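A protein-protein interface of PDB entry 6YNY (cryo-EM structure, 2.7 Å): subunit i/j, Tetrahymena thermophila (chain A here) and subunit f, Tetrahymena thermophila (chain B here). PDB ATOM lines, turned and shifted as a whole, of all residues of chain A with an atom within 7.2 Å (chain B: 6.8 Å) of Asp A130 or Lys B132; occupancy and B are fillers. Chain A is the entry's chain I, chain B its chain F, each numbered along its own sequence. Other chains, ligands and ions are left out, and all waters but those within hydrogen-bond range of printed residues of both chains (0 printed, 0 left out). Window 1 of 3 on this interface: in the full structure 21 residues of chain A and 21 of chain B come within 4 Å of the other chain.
The side-chain amino group (NZ) of Lys B132 is in salt-bridge range of the side-chain carboxylate (OD2) of Asp A130, at 2.9 Å.
Hydrophobic or aromatic side chains of chain A that line the printed part of chain B: Met A131 and Ala A132.
Along chain A the printed residues that touch a printed residue of chain B span positions 130 to 132.
Printed residues of chain B that touch a printed residue of chain A: Lys B132, Lys B133 and Ala B136.
Hydrophobic or aromatic side chains of chain B within 4 Å of the printed part of chain A: Ala B136.
The backbone carbonyl oxygen (O) of Lys A125 lies within hydrogen-bond range of the backbone NH (N) of Met A131 (3.3 Å).
OG1 of Thr B137 lies within hydrogen-bond range of O of Lys B133, at 3.0 Å.
N of Asp A130 is in hydrogen-bond range of O of Lys A125, at 2.7 Å.
Among the printed residues, pairs that only touch across the chains: Met A131 with Ala B136 (3.9 Å), Ala A132 with Lys B132 (3.6 Å), Ala A132 with Lys B133 (3.9 Å) and Ala A132 with Ala B136 (3.4 Å).
Asp A130 touches just one residue of chain B: Lys B132.
Printed residues of chain A within 4 Å of Lys B132: Asp A130 and Ala A132.
Printed residues of chain A within 4 Å of Lys B133: Ala A132 (3.9 Å).
Of the printed residues of chain B, Ala A132 touches Lys B132 (3.6 Å), Lys B133 (3.9 Å) and Ala B136 (3.4 Å).
Printed residues of chain B within 4 Å of Met A131: Ala B136 (3.9 Å).
Printed residues of chain A within 4 Å of Ala B136: Met A131 (3.9 Å) and Ala A132 (3.4 Å).
Ala B129 touches none of the printed residues of chain A.
Gly A129 touches none of the printed residues of chain B.
The nearest printed residue of chain B that does not touch Met A131 is Tyr B135 (4.4 Å).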
ATOM      1  N   PRO A 122      -6.967   6.566   4.511  1.00  0.00           N
ATOM      2  CA  PRO A 122      -7.012   5.180   5.005  1.00  0.00           C
ATOM      3  C   PRO A 122      -7.310   4.150   3.937  1.00  0.00           C
ATOM      4  O   PRO A 122      -6.959   2.978   4.119  1.00  0.00           O
ATOM      5  CB  PRO A 122      -8.123   5.225   6.060  1.00  0.00           C
ATOM      6  CG  PRO A 122      -8.213   6.631   6.454  1.00  0.00           C
ATOM      7  CD  PRO A 122      -7.911   7.422   5.238  1.00  0.00           C
ATOM      8  N   LEU A 124      -5.979   4.037   0.922  1.00  0.00           N
ATOM      9  CA  LEU A 124      -4.706   3.680   0.309  1.00  0.00           C
ATOM     10  C   LEU A 124      -3.972   2.633   1.130  1.00  0.00           C
ATOM     11  O   LEU A 124      -3.336   1.729   0.576  1.00  0.00           O
ATOM     12  CB  LEU A 124      -3.845   4.927   0.146  1.00  0.00           C
ATOM     13  CG  LEU A 124      -3.636   5.474  -1.257  1.00  0.00           C
ATOM     14  CD1 LEU A 124      -4.935   5.597  -1.995  1.00  0.00           C
ATOM     15  CD2 LEU A 124      -2.967   6.812  -1.147  1.00  0.00           C
ATOM     16  N   LYS A 125      -4.042   2.738   2.455  1.00  0.00           N
ATOM     17  CA  LYS A 125      -3.358   1.772   3.306  1.00  0.00           C
ATOM     18  C   LYS A 125      -3.989   0.392   3.199  1.00  0.00           C
ATOM     19  O   LYS A 125      -3.283  -0.622   3.220  1.00  0.00           O
ATOM     20  CB  LYS A 125      -3.368   2.254   4.752  1.00  0.00           C
ATOM     21  CG  LYS A 125      -2.600   3.531   4.979  1.00  0.00           C
ATOM     22  CD  LYS A 125      -2.344   3.781   6.447  1.00  0.00           C
ATOM     23  CE  LYS A 125      -3.627   3.949   7.221  1.00  0.00           C
ATOM     24  NZ  LYS A 125      -3.359   4.236   8.638  1.00  0.00           N
ATOM     25  N   LYS A 126      -5.314   0.328   3.087  1.00  0.00           N
ATOM     26  CA  LYS A 126      -5.974  -0.963   2.958  1.00  0.00           C
ATOM     27  C   LYS A 126      -5.604  -1.644   1.648  1.00  0.00           C
ATOM     28  O   LYS A 126      -5.417  -2.865   1.609  1.00  0.00           O
ATOM     29  CB  LYS A 126      -7.484  -0.792   3.073  1.00  0.00           C
ATOM     30  CG  LYS A 126      -7.968  -0.640   4.500  1.00  0.00           C
ATOM     31  CD  LYS A 126      -9.477  -0.653   4.589  1.00  0.00           C
ATOM     32  CE  LYS A 126     -10.041   0.729   4.786  1.00  0.00           C
ATOM     33  NZ  LYS A 126      -9.687   1.277   6.120  1.00  0.00           N
ATOM     34  N   ARG A 127      -5.493  -0.877   0.567  1.00  0.00           N
ATOM     35  CA  ARG A 127      -5.118  -1.453  -0.713  1.00  0.00           C
ATOM     36  C   ARG A 127      -3.629  -1.748  -0.800  1.00  0.00           C
ATOM     37  O   ARG A 127      -3.215  -2.536  -1.656  1.00  0.00           O
ATOM     38  CB  ARG A 127      -5.527  -0.518  -1.847  1.00  0.00           C
ATOM     39  CG  ARG A 127      -6.972  -0.071  -1.793  1.00  0.00           C
ATOM     40  CD  ARG A 127      -7.941  -1.229  -1.710  1.00  0.00           C
ATOM     41  NE  ARG A 127      -7.696  -2.232  -2.738  1.00  0.00           N
ATOM     42  CZ  ARG A 127      -8.091  -2.118  -3.998  1.00  0.00           C
ATOM     43  NH1 ARG A 127      -8.749  -1.043  -4.394  1.00  0.00           N
ATOM     44  NH2 ARG A 127      -7.823  -3.078  -4.865  1.00  0.00           N
ATOM     45  N   ALA A 128      -2.820  -1.134   0.056  1.00  0.00           N
ATOM     46  CA  ALA A 128      -1.400  -1.430   0.139  1.00  0.00           C
ATOM     47  C   ALA A 128      -1.094  -2.548   1.127  1.00  0.00           C
ATOM     48  O   ALA A 128       0.065  -2.718   1.513  1.00  0.00           O
ATOM     49  CB  ALA A 128      -0.622  -0.174   0.523  1.00  0.00           C
ATOM     50  N   GLY A 129      -2.103  -3.305   1.543  1.00  0.00           N
ATOM     51  CA  GLY A 129      -1.897  -4.390   2.481  1.00  0.00           C
ATOM     52  C   GLY A 129      -1.879  -3.969   3.930  1.00  0.00           C
ATOM     53  O   GLY A 129      -1.109  -4.523   4.722  1.00  0.00           O
ATOM     54  N   ASP A 130      -2.713  -3.004   4.301  1.00  0.00           N
ATOM     55  CA  ASP A 130      -2.735  -2.455   5.653  1.00  0.00           C
ATOM     56  C   ASP A 130      -1.325  -2.063   6.085  1.00  0.00           C
ATOM     57  O   ASP A 130      -0.788  -2.533   7.089  1.00  0.00           O
ATOM     58  CB  ASP A 130      -3.359  -3.441   6.638  1.00  0.00           C
ATOM     59  CG  ASP A 130      -3.521  -2.850   8.022  1.00  0.00           C
ATOM     60  OD1 ASP A 130      -4.262  -1.856   8.158  1.00  0.00           O
ATOM     61  OD2 ASP A 130      -2.909  -3.377   8.974  1.00  0.00           O
ATOM     62  N   MET A 131      -0.730  -1.185   5.291  1.00  0.00           N
ATOM     63  CA  MET A 131       0.657  -0.787   5.451  1.00  0.00           C
ATOM     64  C   MET A 131       0.743   0.724   5.591  1.00  0.00           C
ATOM     65  O   MET A 131      -0.001   1.464   4.940  1.00  0.00           O
ATOM     66  CB  MET A 131       1.481  -1.260   4.258  1.00  0.00           C
ATOM     67  CG  MET A 131       2.970  -1.165   4.439  1.00  0.00           C
ATOM     68  SD  MET A 131       3.854  -2.016   3.126  1.00  0.00           S
ATOM     69  CE  MET A 131       5.526  -1.534   3.518  1.00  0.00           C
ATOM     70  N   ALA A 132       1.652   1.175   6.448  1.00  0.00           N
ATOM     71  CA  ALA A 132       1.801   2.597   6.702  1.00  0.00           C
ATOM     72  C   ALA A 132       2.411   3.293   5.494  1.00  0.00           C
ATOM     73  O   ALA A 132       3.368   2.803   4.890  1.00  0.00           O
ATOM     74  CB  ALA A 132       2.667   2.827   7.935  1.00  0.00           C
ATOM     75  N   LEU A 133       1.849   4.438   5.144  1.00  0.00           N
ATOM     76  CA  LEU A 133       2.299   5.240   4.021  1.00  0.00           C
ATOM     77  C   LEU A 133       2.538   6.668   4.473  1.00  0.00           C
ATOM     78  O   LEU A 133       2.008   7.102   5.501  1.00  0.00           O
ATOM     79  CB  LEU A 133       1.258   5.236   2.894  1.00  0.00           C
ATOM     80  CG  LEU A 133       0.834   3.874   2.361  1.00  0.00           C
ATOM     81  CD1 LEU A 133      -0.394   4.011   1.510  1.00  0.00           C
ATOM     82  CD2 LEU A 133       1.957   3.261   1.569  1.00  0.00           C
ATOM     83  N   SER B 127       0.635   1.868  19.779  1.00  0.00           N
ATOM     84  CA  SER B 127       1.873   1.104  19.710  1.00  0.00           C
ATOM     85  C   SER B 127       1.856   0.130  18.545  1.00  0.00           C
ATOM     86  O   SER B 127       2.902  -0.143  17.948  1.00  0.00           O
ATOM     87  CB  SER B 127       2.096   0.360  21.024  1.00  0.00           C
ATOM     88  OG  SER B 127       3.385  -0.214  21.074  1.00  0.00           O
ATOM     89  N   ILE B 128       0.683  -0.405  18.214  1.00  0.00           N
ATOM     90  CA  ILE B 128       0.557  -1.278  17.055  1.00  0.00           C
ATOM     91  C   ILE B 128       0.735  -0.484  15.771  1.00  0.00           C
ATOM     92  O   ILE B 128       1.377  -0.947  14.822  1.00  0.00           O
ATOM     93  CB  ILE B 128      -0.797  -2.004  17.088  1.00  0.00           C
ATOM     94  CG1 ILE B 128      -0.865  -2.941  18.287  1.00  0.00           C
ATOM     95  CG2 ILE B 128      -1.020  -2.777  15.810  1.00  0.00           C
ATOM     96  CD1 ILE B 128      -2.227  -3.484  18.530  1.00  0.00           C
ATOM     97  N   ALA B 129       0.166   0.719  15.716  1.00  0.00           N
ATOM     98  CA  ALA B 129       0.312   1.551  14.531  1.00  0.00           C
ATOM     99  C   ALA B 129       1.760   1.972  14.324  1.00  0.00           C
ATOM    100  O   ALA B 129       2.225   2.070  13.183  1.00  0.00           O
ATOM    101  CB  ALA B 129      -0.595   2.770  14.638  1.00  0.00           C
ATOM    102  N   TYR B 130       2.491   2.230  15.409  1.00  0.00           N
ATOM    103  CA  TYR B 130       3.897   2.582  15.266  1.00  0.00           C
ATOM    104  C   TYR B 130       4.718   1.396  14.782  1.00  0.00           C
ATOM    105  O   TYR B 130       5.704   1.581  14.063  1.00  0.00           O
ATOM    106  CB  TYR B 130       4.455   3.110  16.586  1.00  0.00           C
ATOM    107  CG  TYR B 130       5.841   3.692  16.463  1.00  0.00           C
ATOM    108  CD1 TYR B 130       6.029   5.010  16.082  1.00  0.00           C
ATOM    109  CD2 TYR B 130       6.962   2.925  16.721  1.00  0.00           C
ATOM    110  CE1 TYR B 130       7.287   5.543  15.966  1.00  0.00           C
ATOM    111  CE2 TYR B 130       8.223   3.449  16.608  1.00  0.00           C
ATOM    112  CZ  TYR B 130       8.383   4.758  16.226  1.00  0.00           C
ATOM    113  OH  TYR B 130       9.646   5.285  16.114  1.00  0.00           O
ATOM    114  N   SER B 131       4.329   0.180  15.162  1.00  0.00           N
ATOM    115  CA  SER B 131       5.017  -1.000  14.657  1.00  0.00           C
ATOM    116  C   SER B 131       4.855  -1.133  13.151  1.00  0.00           C
ATOM    117  O   SER B 131       5.760  -1.624  12.470  1.00  0.00           O
ATOM    118  CB  SER B 131       4.493  -2.250  15.359  1.00  0.00           C
ATOM    119  OG  SER B 131       3.188  -2.573  14.930  1.00  0.00           O
ATOM    120  N   LYS B 132       3.713  -0.702  12.616  1.00  0.00           N
ATOM    121  CA  LYS B 132       3.530  -0.689  11.170  1.00  0.00           C
ATOM    122  C   LYS B 132       4.337   0.420  10.514  1.00  0.00           C
ATOM    123  O   LYS B 132       4.748   0.283   9.356  1.00  0.00           O
ATOM    124  CB  LYS B 132       2.052  -0.543  10.833  1.00  0.00           C
ATOM    125  CG  LYS B 132       1.216  -1.725  11.253  1.00  0.00           C
ATOM    126  CD  LYS B 132      -0.247  -1.513  10.950  1.00  0.00           C
ATOM    127  CE  LYS B 132      -1.085  -2.678  11.433  1.00  0.00           C
ATOM    128  NZ  LYS B 132      -0.704  -3.950  10.766  1.00  0.00           N
ATOM    129  N   LYS B 133       4.570   1.520  11.228  1.00  0.00           N
ATOM    130  CA  LYS B 133       5.453   2.560  10.715  1.00  0.00           C
ATOM    131  C   LYS B 133       6.886   2.061  10.630  1.00  0.00           C
ATOM    132  O   LYS B 133       7.603   2.371   9.674  1.00  0.00           O
ATOM    133  CB  LYS B 133       5.363   3.801  11.600  1.00  0.00           C
ATOM    134  CG  LYS B 133       6.552   4.723  11.521  1.00  0.00           C
ATOM    135  CD  LYS B 133       6.325   5.985  12.311  1.00  0.00           C
ATOM    136  CE  LYS B 133       7.561   6.855  12.313  1.00  0.00           C
ATOM    137  NZ  LYS B 133       7.324   8.181  12.949  1.00  0.00           N
ATOM    138  N   GLN B 134       7.319   1.285  11.622  1.00  0.00           N
ATOM    139  CA  GLN B 134       8.670   0.747  11.600  1.00  0.00           C
ATOM    140  C   GLN B 134       8.826  -0.331  10.538  1.00  0.00           C
ATOM    141  O   GLN B 134       9.918  -0.498   9.986  1.00  0.00           O
ATOM    142  CB  GLN B 134       9.038   0.201  12.979  1.00  0.00           C
ATOM    143  CG  GLN B 134       9.425   1.266  13.979  1.00  0.00           C
ATOM    144  CD  GLN B 134      10.043   0.696  15.237  1.00  0.00           C
ATOM    145  OE1 GLN B 134      11.081   1.167  15.699  1.00  0.00           O
ATOM    146  NE2 GLN B 134       9.405  -0.318  15.803  1.00  0.00           N
ATOM    147  N   TYR B 135       7.756  -1.066  10.235  1.00  0.00           N
ATOM    148  CA  TYR B 135       7.831  -2.055   9.168  1.00  0.00           C
ATOM    149  C   TYR B 135       7.927  -1.384   7.807  1.00  0.00           C
ATOM    150  O   TYR B 135       8.691  -1.826   6.943  1.00  0.00           O
ATOM    151  CB  TYR B 135       6.625  -2.990   9.222  1.00  0.00           C
ATOM    152  CG  TYR B 135       6.672  -4.067   8.169  1.00  0.00           C
ATOM    153  CD1 TYR B 135       7.568  -5.113   8.268  1.00  0.00           C
ATOM    154  CD2 TYR B 135       5.825  -4.035   7.076  1.00  0.00           C
ATOM    155  CE1 TYR B 135       7.623  -6.092   7.312  1.00  0.00           C
ATOM    156  CE2 TYR B 135       5.872  -5.010   6.114  1.00  0.00           C
ATOM    157  CZ  TYR B 135       6.773  -6.038   6.236  1.00  0.00           C
ATOM    158  OH  TYR B 135       6.821  -7.016   5.277  1.00  0.00           O
ATOM    159  N   ALA B 136       7.163  -0.313   7.598  1.00  0.00           N
ATOM    160  CA  ALA B 136       7.283   0.448   6.362  1.00  0.00           C
ATOM    161  C   ALA B 136       8.658   1.087   6.250  1.00  0.00           C
ATOM    162  O   ALA B 136       9.261   1.099   5.172  1.00  0.00           O
ATOM    163  CB  ALA B 136       6.193   1.514   6.292  1.00  0.00           C
ATOM    164  N   THR B 137       9.167   1.626   7.357  1.00  0.00           N
ATOM    165  CA  THR B 137      10.520   2.166   7.369  1.00  0.00           C
ATOM    166  C   THR B 137      11.544   1.085   7.053  1.00  0.00           C
ATOM    167  O   THR B 137      12.522   1.334   6.341  1.00  0.00           O
ATOM    168  CB  THR B 137      10.806   2.802   8.727  1.00  0.00           C
ATOM    169  OG1 THR B 137       9.977   3.956   8.902  1.00  0.00           O
ATOM    170  CG2 THR B 137      12.253   3.203   8.846  1.00  0.00           C
